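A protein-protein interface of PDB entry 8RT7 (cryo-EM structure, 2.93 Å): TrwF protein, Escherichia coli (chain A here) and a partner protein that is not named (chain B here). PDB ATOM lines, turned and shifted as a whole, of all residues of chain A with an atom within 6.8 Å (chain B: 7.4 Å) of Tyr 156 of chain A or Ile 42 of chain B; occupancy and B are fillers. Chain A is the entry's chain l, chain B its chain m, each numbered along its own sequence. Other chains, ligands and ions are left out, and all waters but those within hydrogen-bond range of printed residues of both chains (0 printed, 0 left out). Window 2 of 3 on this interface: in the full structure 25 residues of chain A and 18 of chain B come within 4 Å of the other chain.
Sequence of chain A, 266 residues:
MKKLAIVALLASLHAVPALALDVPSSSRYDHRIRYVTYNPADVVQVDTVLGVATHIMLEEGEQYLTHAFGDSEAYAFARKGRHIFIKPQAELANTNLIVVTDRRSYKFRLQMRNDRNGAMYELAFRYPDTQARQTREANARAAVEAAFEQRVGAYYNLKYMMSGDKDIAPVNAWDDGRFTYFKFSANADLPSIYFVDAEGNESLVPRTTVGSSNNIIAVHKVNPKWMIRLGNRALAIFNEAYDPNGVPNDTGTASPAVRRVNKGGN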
ATOM      1  N   ARG A 151     -13.087   3.287 -32.327  1.00  0.00           N
ATOM      2  CA  ARG A 151     -13.986   2.662 -31.344  1.00  0.00           C
ATOM      3  C   ARG A 151     -13.624   3.046 -29.909  1.00  0.00           C
ATOM      4  O   ARG A 151     -13.350   2.204 -29.052  1.00  0.00           O
ATOM      5  CB  ARG A 151     -14.044   1.137 -31.517  1.00  0.00           C
ATOM      6  CG  ARG A 151     -12.729   0.378 -31.424  1.00  0.00           C
ATOM      7  CD  ARG A 151     -12.921  -0.954 -30.720  1.00  0.00           C
ATOM      8  NE  ARG A 151     -11.769  -1.836 -30.883  1.00  0.00           N
ATOM      9  CZ  ARG A 151     -10.723  -1.867 -30.061  1.00  0.00           C
ATOM     10  NH1 ARG A 151     -10.670  -1.062 -29.011  1.00  0.00           N
ATOM     11  NH2 ARG A 151      -9.722  -2.704 -30.294  1.00  0.00           N
ATOM     12  N   ALA A 154     -15.909   2.986 -25.222  1.00  0.00           N
ATOM     13  CA  ALA A 154     -16.833   1.863 -25.249  1.00  0.00           C
ATOM     14  C   ALA A 154     -16.801   1.125 -23.920  1.00  0.00           C
ATOM     15  O   ALA A 154     -15.734   0.943 -23.326  1.00  0.00           O
ATOM     16  CB  ALA A 154     -16.497   0.904 -26.393  1.00  0.00           C
ATOM     17  N   TYR A 155     -17.972   0.714 -23.453  1.00  0.00           N
ATOM     18  CA  TYR A 155     -18.106  -0.056 -22.228  1.00  0.00           C
ATOM     19  C   TYR A 155     -18.394  -1.505 -22.582  1.00  0.00           C
ATOM     20  O   TYR A 155     -19.304  -1.786 -23.367  1.00  0.00           O
ATOM     21  CB  TYR A 155     -19.224   0.499 -21.348  1.00  0.00           C
ATOM     22  CG  TYR A 155     -19.749  -0.491 -20.336  1.00  0.00           C
ATOM     23  CD1 TYR A 155     -18.967  -0.898 -19.263  1.00  0.00           C
ATOM     24  CD2 TYR A 155     -21.021  -1.027 -20.458  1.00  0.00           C
ATOM     25  CE1 TYR A 155     -19.442  -1.807 -18.335  1.00  0.00           C
ATOM     26  CE2 TYR A 155     -21.505  -1.938 -19.536  1.00  0.00           C
ATOM     27  CZ  TYR A 155     -20.711  -2.325 -18.478  1.00  0.00           C
ATOM     28  OH  TYR A 155     -21.193  -3.229 -17.562  1.00  0.00           O
ATOM     29  N   TYR A 156     -17.628  -2.420 -21.996  1.00  0.00           N
ATOM     30  CA  TYR A 156     -17.708  -3.838 -22.305  1.00  0.00           C
ATOM     31  C   TYR A 156     -18.348  -4.582 -21.144  1.00  0.00           C
ATOM     32  O   TYR A 156     -18.000  -4.347 -19.985  1.00  0.00           O
ATOM     33  CB  TYR A 156     -16.322  -4.408 -22.587  1.00  0.00           C
ATOM     34  CG  TYR A 156     -15.621  -3.767 -23.752  1.00  0.00           C
ATOM     35  CD1 TYR A 156     -16.005  -4.036 -25.051  1.00  0.00           C
ATOM     36  CD2 TYR A 156     -14.572  -2.893 -23.553  1.00  0.00           C
ATOM     37  CE1 TYR A 156     -15.364  -3.456 -26.115  1.00  0.00           C
ATOM     38  CE2 TYR A 156     -13.925  -2.308 -24.613  1.00  0.00           C
ATOM     39  CZ  TYR A 156     -14.325  -2.593 -25.891  1.00  0.00           C
ATOM     40  OH  TYR A 156     -13.684  -2.011 -26.954  1.00  0.00           O
ATOM     41  N   ASN A 157     -19.277  -5.473 -21.460  1.00  0.00           N
ATOM     42  CA  ASN A 157     -19.950  -6.306 -20.474  1.00  0.00           C
ATOM     43  C   ASN A 157     -19.381  -7.710 -20.576  1.00  0.00           C
ATOM     44  O   ASN A 157     -19.422  -8.318 -21.646  1.00  0.00           O
ATOM     45  CB  ASN A 157     -21.460  -6.310 -20.708  1.00  0.00           C
ATOM     46  CG  ASN A 157     -22.197  -7.210 -19.748  1.00  0.00           C
ATOM     47  OD1 ASN A 157     -21.796  -7.363 -18.602  1.00  0.00           O
ATOM     48  ND2 ASN A 157     -23.291  -7.795 -20.204  1.00  0.00           N
ATOM     49  N   LEU A 158     -18.849  -8.222 -19.470  1.00  0.00           N
ATOM     50  CA  LEU A 158     -18.240  -9.544 -19.444  1.00  0.00           C
ATOM     51  C   LEU A 158     -18.954 -10.495 -18.498  1.00  0.00           C
ATOM     52  O   LEU A 158     -18.420 -11.565 -18.198  1.00  0.00           O
ATOM     53  CB  LEU A 158     -16.766  -9.444 -19.047  1.00  0.00           C
ATOM     54  CG  LEU A 158     -15.808  -8.788 -20.034  1.00  0.00           C
ATOM     55  CD1 LEU A 158     -14.611  -8.242 -19.306  1.00  0.00           C
ATOM     56  CD2 LEU A 158     -15.373  -9.790 -21.063  1.00  0.00           C
ATOM     57  N   LYS A 159     -20.140 -10.134 -18.014  1.00  0.00           N
ATOM     58  CA  LYS A 159     -20.891 -10.981 -17.090  1.00  0.00           C
ATOM     59  C   LYS A 159     -21.718 -11.966 -17.903  1.00  0.00           C
ATOM     60  O   LYS A 159     -22.926 -11.822 -18.075  1.00  0.00           O
ATOM     61  CB  LYS A 159     -21.767 -10.135 -16.179  1.00  0.00           C
ATOM     62  CG  LYS A 159     -21.002  -9.176 -15.296  1.00  0.00           C
ATOM     63  CD  LYS A 159     -20.389  -9.889 -14.113  1.00  0.00           C
ATOM     64  CE  LYS A 159     -19.002  -9.360 -13.818  1.00  0.00           C
ATOM     65  NZ  LYS A 159     -18.047  -9.696 -14.905  1.00  0.00           N
ATOM     66  N   ALA A 173     -16.897 -14.454 -24.195  1.00  0.00           N
ATOM     67  CA  ALA A 173     -18.088 -13.776 -24.683  1.00  0.00           C
ATOM     68  C   ALA A 173     -18.239 -12.446 -23.961  1.00  0.00           C
ATOM     69  O   ALA A 173     -18.001 -12.356 -22.756  1.00  0.00           O
ATOM     70  CB  ALA A 173     -19.342 -14.627 -24.490  1.00  0.00           C
ATOM     71  N   TRP A 174     -18.626 -11.419 -24.707  1.00  0.00           N
ATOM     72  CA  TRP A 174     -18.786 -10.078 -24.163  1.00  0.00           C
ATOM     73  C   TRP A 174     -19.711  -9.299 -25.085  1.00  0.00           C
ATOM     74  O   TRP A 174     -20.115  -9.785 -26.140  1.00  0.00           O
ATOM     75  CB  TRP A 174     -17.434  -9.376 -23.998  1.00  0.00           C
ATOM     76  CG  TRP A 174     -16.770  -8.964 -25.278  1.00  0.00           C
ATOM     77  CD1 TRP A 174     -16.795  -7.736 -25.849  1.00  0.00           C
ATOM     78  CD2 TRP A 174     -15.965  -9.783 -26.129  1.00  0.00           C
ATOM     79  NE1 TRP A 174     -16.068  -7.733 -27.005  1.00  0.00           N
ATOM     80  CE2 TRP A 174     -15.549  -8.983 -27.201  1.00  0.00           C
ATOM     81  CE3 TRP A 174     -15.561 -11.115 -26.091  1.00  0.00           C
ATOM     82  CZ2 TRP A 174     -14.751  -9.471 -28.222  1.00  0.00           C
ATOM     83  CZ3 TRP A 174     -14.775 -11.596 -27.107  1.00  0.00           C
ATOM     84  CH2 TRP A 174     -14.378 -10.780 -28.156  1.00  0.00           C
ATOM     85  N   ASP A 175     -20.063  -8.085 -24.665  1.00  0.00           N
ATOM     86  CA  ASP A 175     -20.758  -7.166 -25.553  1.00  0.00           C
ATOM     87  C   ASP A 175     -20.351  -5.738 -25.232  1.00  0.00           C
ATOM     88  O   ASP A 175     -19.945  -5.428 -24.114  1.00  0.00           O
ATOM     89  CB  ASP A 175     -22.282  -7.314 -25.479  1.00  0.00           C
ATOM     90  CG  ASP A 175     -22.842  -7.013 -24.123  1.00  0.00           C
ATOM     91  OD1 ASP A 175     -22.846  -5.837 -23.717  1.00  0.00           O
ATOM     92  OD2 ASP A 175     -23.314  -7.959 -23.469  1.00  0.00           O
ATOM     93  N   ASP A 176     -20.459  -4.875 -26.237  1.00  0.00           N
ATOM     94  CA  ASP A 176     -20.094  -3.472 -26.130  1.00  0.00           C
ATOM     95  C   ASP A 176     -21.303  -2.564 -25.950  1.00  0.00           C
ATOM     96  O   ASP A 176     -21.179  -1.346 -26.094  1.00  0.00           O
ATOM     97  CB  ASP A 176     -19.308  -3.044 -27.366  1.00  0.00           C
ATOM     98  CG  ASP A 176     -20.062  -3.307 -28.648  1.00  0.00           C
ATOM     99  OD1 ASP A 176     -21.193  -3.811 -28.576  1.00  0.00           O
ATOM    100  OD2 ASP A 176     -19.536  -3.005 -29.733  1.00  0.00           O
ATOM    101  N   GLY A 177     -22.466  -3.128 -25.644  1.00  0.00           N
ATOM    102  CA  GLY A 177     -23.695  -2.384 -25.572  1.00  0.00           C
ATOM    103  C   GLY A 177     -24.450  -2.313 -26.876  1.00  0.00           C
ATOM    104  O   GLY A 177     -25.616  -1.916 -26.882  1.00  0.00           O
ATOM    105  N   TYR A 181     -20.360 -10.460 -28.767  1.00  0.00           N
ATOM    106  CA  TYR A 181     -19.268 -11.170 -29.417  1.00  0.00           C
ATOM    107  C   TYR A 181     -18.983 -12.476 -28.699  1.00  0.00           C
ATOM    108  O   TYR A 181     -18.807 -12.490 -27.481  1.00  0.00           O
ATOM    109  CB  TYR A 181     -18.000 -10.334 -29.442  1.00  0.00           C
ATOM    110  CG  TYR A 181     -18.184  -8.964 -30.006  1.00  0.00           C
ATOM    111  CD1 TYR A 181     -17.957  -8.709 -31.339  1.00  0.00           C
ATOM    112  CD2 TYR A 181     -18.566  -7.919 -29.200  1.00  0.00           C
ATOM    113  CE1 TYR A 181     -18.119  -7.460 -31.850  1.00  0.00           C
ATOM    114  CE2 TYR A 181     -18.727  -6.670 -29.702  1.00  0.00           C
ATOM    115  CZ  TYR A 181     -18.504  -6.443 -31.026  1.00  0.00           C
ATOM    116  OH  TYR A 181     -18.668  -5.185 -31.535  1.00  0.00           O
ATOM    117  N   ASN B  35     -16.073 -16.490 -19.501  1.00  0.00           N
ATOM    118  CA  ASN B  35     -14.791 -15.801 -19.570  1.00  0.00           C
ATOM    119  C   ASN B  35     -13.912 -16.283 -18.429  1.00  0.00           C
ATOM    120  O   ASN B  35     -14.029 -15.813 -17.297  1.00  0.00           O
ATOM    121  CB  ASN B  35     -14.991 -14.294 -19.511  1.00  0.00           C
ATOM    122  CG  ASN B  35     -15.685 -13.757 -20.732  1.00  0.00           C
ATOM    123  OD1 ASN B  35     -15.050 -13.474 -21.736  1.00  0.00           O
ATOM    124  ND2 ASN B  35     -16.996 -13.617 -20.653  1.00  0.00           N
ATOM    125  N   VAL B  38      -9.796 -12.411 -19.400  1.00  0.00           N
ATOM    126  CA  VAL B  38     -10.271 -11.244 -20.148  1.00  0.00           C
ATOM    127  C   VAL B  38      -9.816 -11.360 -21.598  1.00  0.00           C
ATOM    128  O   VAL B  38      -8.646 -11.691 -21.851  1.00  0.00           O
ATOM    129  CB  VAL B  38      -9.752  -9.958 -19.510  1.00  0.00           C
ATOM    130  CG1 VAL B  38     -10.322  -8.753 -20.217  1.00  0.00           C
ATOM    131  CG2 VAL B  38     -10.115  -9.926 -18.044  1.00  0.00           C
ATOM    132  N   PRO B  39     -10.687 -11.108 -22.572  1.00  0.00           N
ATOM    133  CA  PRO B  39     -10.277 -11.203 -23.974  1.00  0.00           C
ATOM    134  C   PRO B  39      -9.236 -10.154 -24.335  1.00  0.00           C
ATOM    135  O   PRO B  39      -9.049  -9.151 -23.646  1.00  0.00           O
ATOM    136  CB  PRO B  39     -11.579 -10.971 -24.744  1.00  0.00           C
ATOM    137  CG  PRO B  39     -12.660 -11.202 -23.760  1.00  0.00           C
ATOM    138  CD  PRO B  39     -12.124 -10.839 -22.431  1.00  0.00           C
ATOM    139  N   VAL B  40      -8.545 -10.413 -25.442  1.00  0.00           N
ATOM    140  CA  VAL B  40      -7.525  -9.484 -25.908  1.00  0.00           C
ATOM    141  C   VAL B  40      -8.132  -8.417 -26.812  1.00  0.00           C
ATOM    142  O   VAL B  40      -7.633  -7.291 -26.867  1.00  0.00           O
ATOM    143  CB  VAL B  40      -6.401 -10.259 -26.614  1.00  0.00           C
ATOM    144  CG1 VAL B  40      -5.393  -9.310 -27.242  1.00  0.00           C
ATOM    145  CG2 VAL B  40      -5.721 -11.195 -25.635  1.00  0.00           C
ATOM    146  N   GLU B  41      -9.220  -8.733 -27.515  1.00  0.00           N
ATOM    147  CA  GLU B  41      -9.886  -7.744 -28.356  1.00  0.00           C
ATOM    148  C   GLU B  41     -10.534  -6.627 -27.554  1.00  0.00           C
ATOM    149  O   GLU B  41     -10.965  -5.633 -28.144  1.00  0.00           O
ATOM    150  CB  GLU B  41     -10.924  -8.418 -29.252  1.00  0.00           C
ATOM    151  CG  GLU B  41     -10.343  -9.429 -30.222  1.00  0.00           C
ATOM    152  CD  GLU B  41      -9.953 -10.740 -29.581  1.00  0.00           C
ATOM    153  OE1 GLU B  41      -9.460 -11.623 -30.312  1.00  0.00           O
ATOM    154  OE2 GLU B  41     -10.137 -10.892 -28.358  1.00  0.00           O
ATOM    155  N   ILE B  42     -10.635  -6.779 -26.231  1.00  0.00           N
ATOM    156  CA  ILE B  42     -10.909  -5.656 -25.348  1.00  0.00           C
ATOM    157  C   ILE B  42      -9.654  -4.832 -25.090  1.00  0.00           C
ATOM    158  O   ILE B  42      -9.724  -3.794 -24.419  1.00  0.00           O
ATOM    159  CB  ILE B  42     -11.547  -6.202 -24.052  1.00  0.00           C
ATOM    160  CG1 ILE B  42     -12.752  -7.069 -24.406  1.00  0.00           C
ATOM    161  CG2 ILE B  42     -11.980  -5.099 -23.113  1.00  0.00           C
ATOM    162  CD1 ILE B  42     -13.639  -7.368 -23.240  1.00  0.00           C
ATOM    163  N   GLN B  43      -8.513  -5.240 -25.653  1.00  0.00           N
ATOM    164  CA  GLN B  43      -7.213  -4.609 -25.402  1.00  0.00           C
ATOM    165  C   GLN B  43      -6.843  -4.698 -23.927  1.00  0.00           C
ATOM    166  O   GLN B  43      -7.226  -3.835 -23.142  1.00  0.00           O
ATOM    167  CB  GLN B  43      -7.184  -3.161 -25.895  1.00  0.00           C
ATOM    168  CG  GLN B  43      -6.354  -2.960 -27.147  1.00  0.00           C
ATOM    169  CD  GLN B  43      -7.004  -3.552 -28.380  1.00  0.00           C
ATOM    170  OE1 GLN B  43      -8.120  -3.187 -28.744  1.00  0.00           O
ATOM    171  NE2 GLN B  43      -6.304  -4.473 -29.031  1.00  0.00           N
ATOM    172  N   ARG B  44      -7.200  -5.821 -23.316  1.00  0.00           N
ATOM    173  CA  ARG B  44      -6.838  -6.107 -21.937  1.00  0.00           C
ATOM    174  C   ARG B  44      -6.170  -7.473 -21.842  1.00  0.00           C
ATOM    175  O   ARG B  44      -5.465  -7.891 -22.759  1.00  0.00           O
ATOM    176  CB  ARG B  44      -8.069  -6.054 -21.032  1.00  0.00           C
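The side-chain amide oxygen (OE1) of Gln 43 of chain B sits close to the guanidinium group (NH1) of Arg 151 of chain A (3.3 Å). The backbone carbonyl oxygen (O) of Ala 173 of chain A sits at hydrogen-bond distance from the side-chain amide nitrogen (ND2) of Asn 35 of chain B (2.7 Å).
Tyr 156 of chain A touches one residue of chain B. Ile 42 of chain B touches two residues of chain A. Printed residues of chain A within 4 Å of Pro 39 of chain B: Leu 158 (3.7 Å) and Trp 174 (3.7 Å). Printed residues of chain B within 4 Å of Leu 158 of chain A: Asn 35, Pro 39 and Ile 42. Of the printed residues of chain A, Glu 41 of chain B touches Arg 151 (3.8 Å). Of the printed residues of chain A, Gln 43 of chain B touches Arg 151 (2.3 Å). Asp 176 of chain A touches none of the printed residues of chain B. Val 40 of chain B touches none of the printed residues of chain A. The nearest residue of chain A that does not touch Ile 42 of chain B is Trp 174 of chain A (4.1 Å).
O of Trp 174 of chain A is in hydrogen-bond range of N of Tyr 181 of chain A (2.7 Å).
Of the 13 printed residues of chain A, 5 touch a printed residue of chain B. Printed residues of chain A that touch a printed residue of chain B: Arg 151, Tyr 156, Leu 158, Ala 173 and Trp 174. Along chain A the printed residues that touch a printed residue of chain B span positions 151 to 174. Hydrophobic or aromatic side chains of chain B within 4 Å of the printed part of chain A: Pro 39 and Ile 42. Along chain B the printed residues that touch a printed residue of chain A span positions 35 to 43. Among the printed residues, no Asp or Glu carboxylate lies within 4 Å of a Lys or Arg side-chain nitrogen of the other chain.
Glu 41 of chain B touches Arg 151 of chain A. CG2 of Ile 42 of chain B touches CD2 of Tyr 156 of chain A, 3.4 Å away. ND2 of Asn 35 of chain B touches O of Leu 158 of chain A, 3.5 Å away. Pro 39 of chain B touches Leu 158 of chain A (CD to CD2, 3.7 Å). CD1 of Ile 42 of chain B touches CD2 of Leu 158 of chain A (3.7 Å). Trp 174 of chain A touches Pro 39 of chain B.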
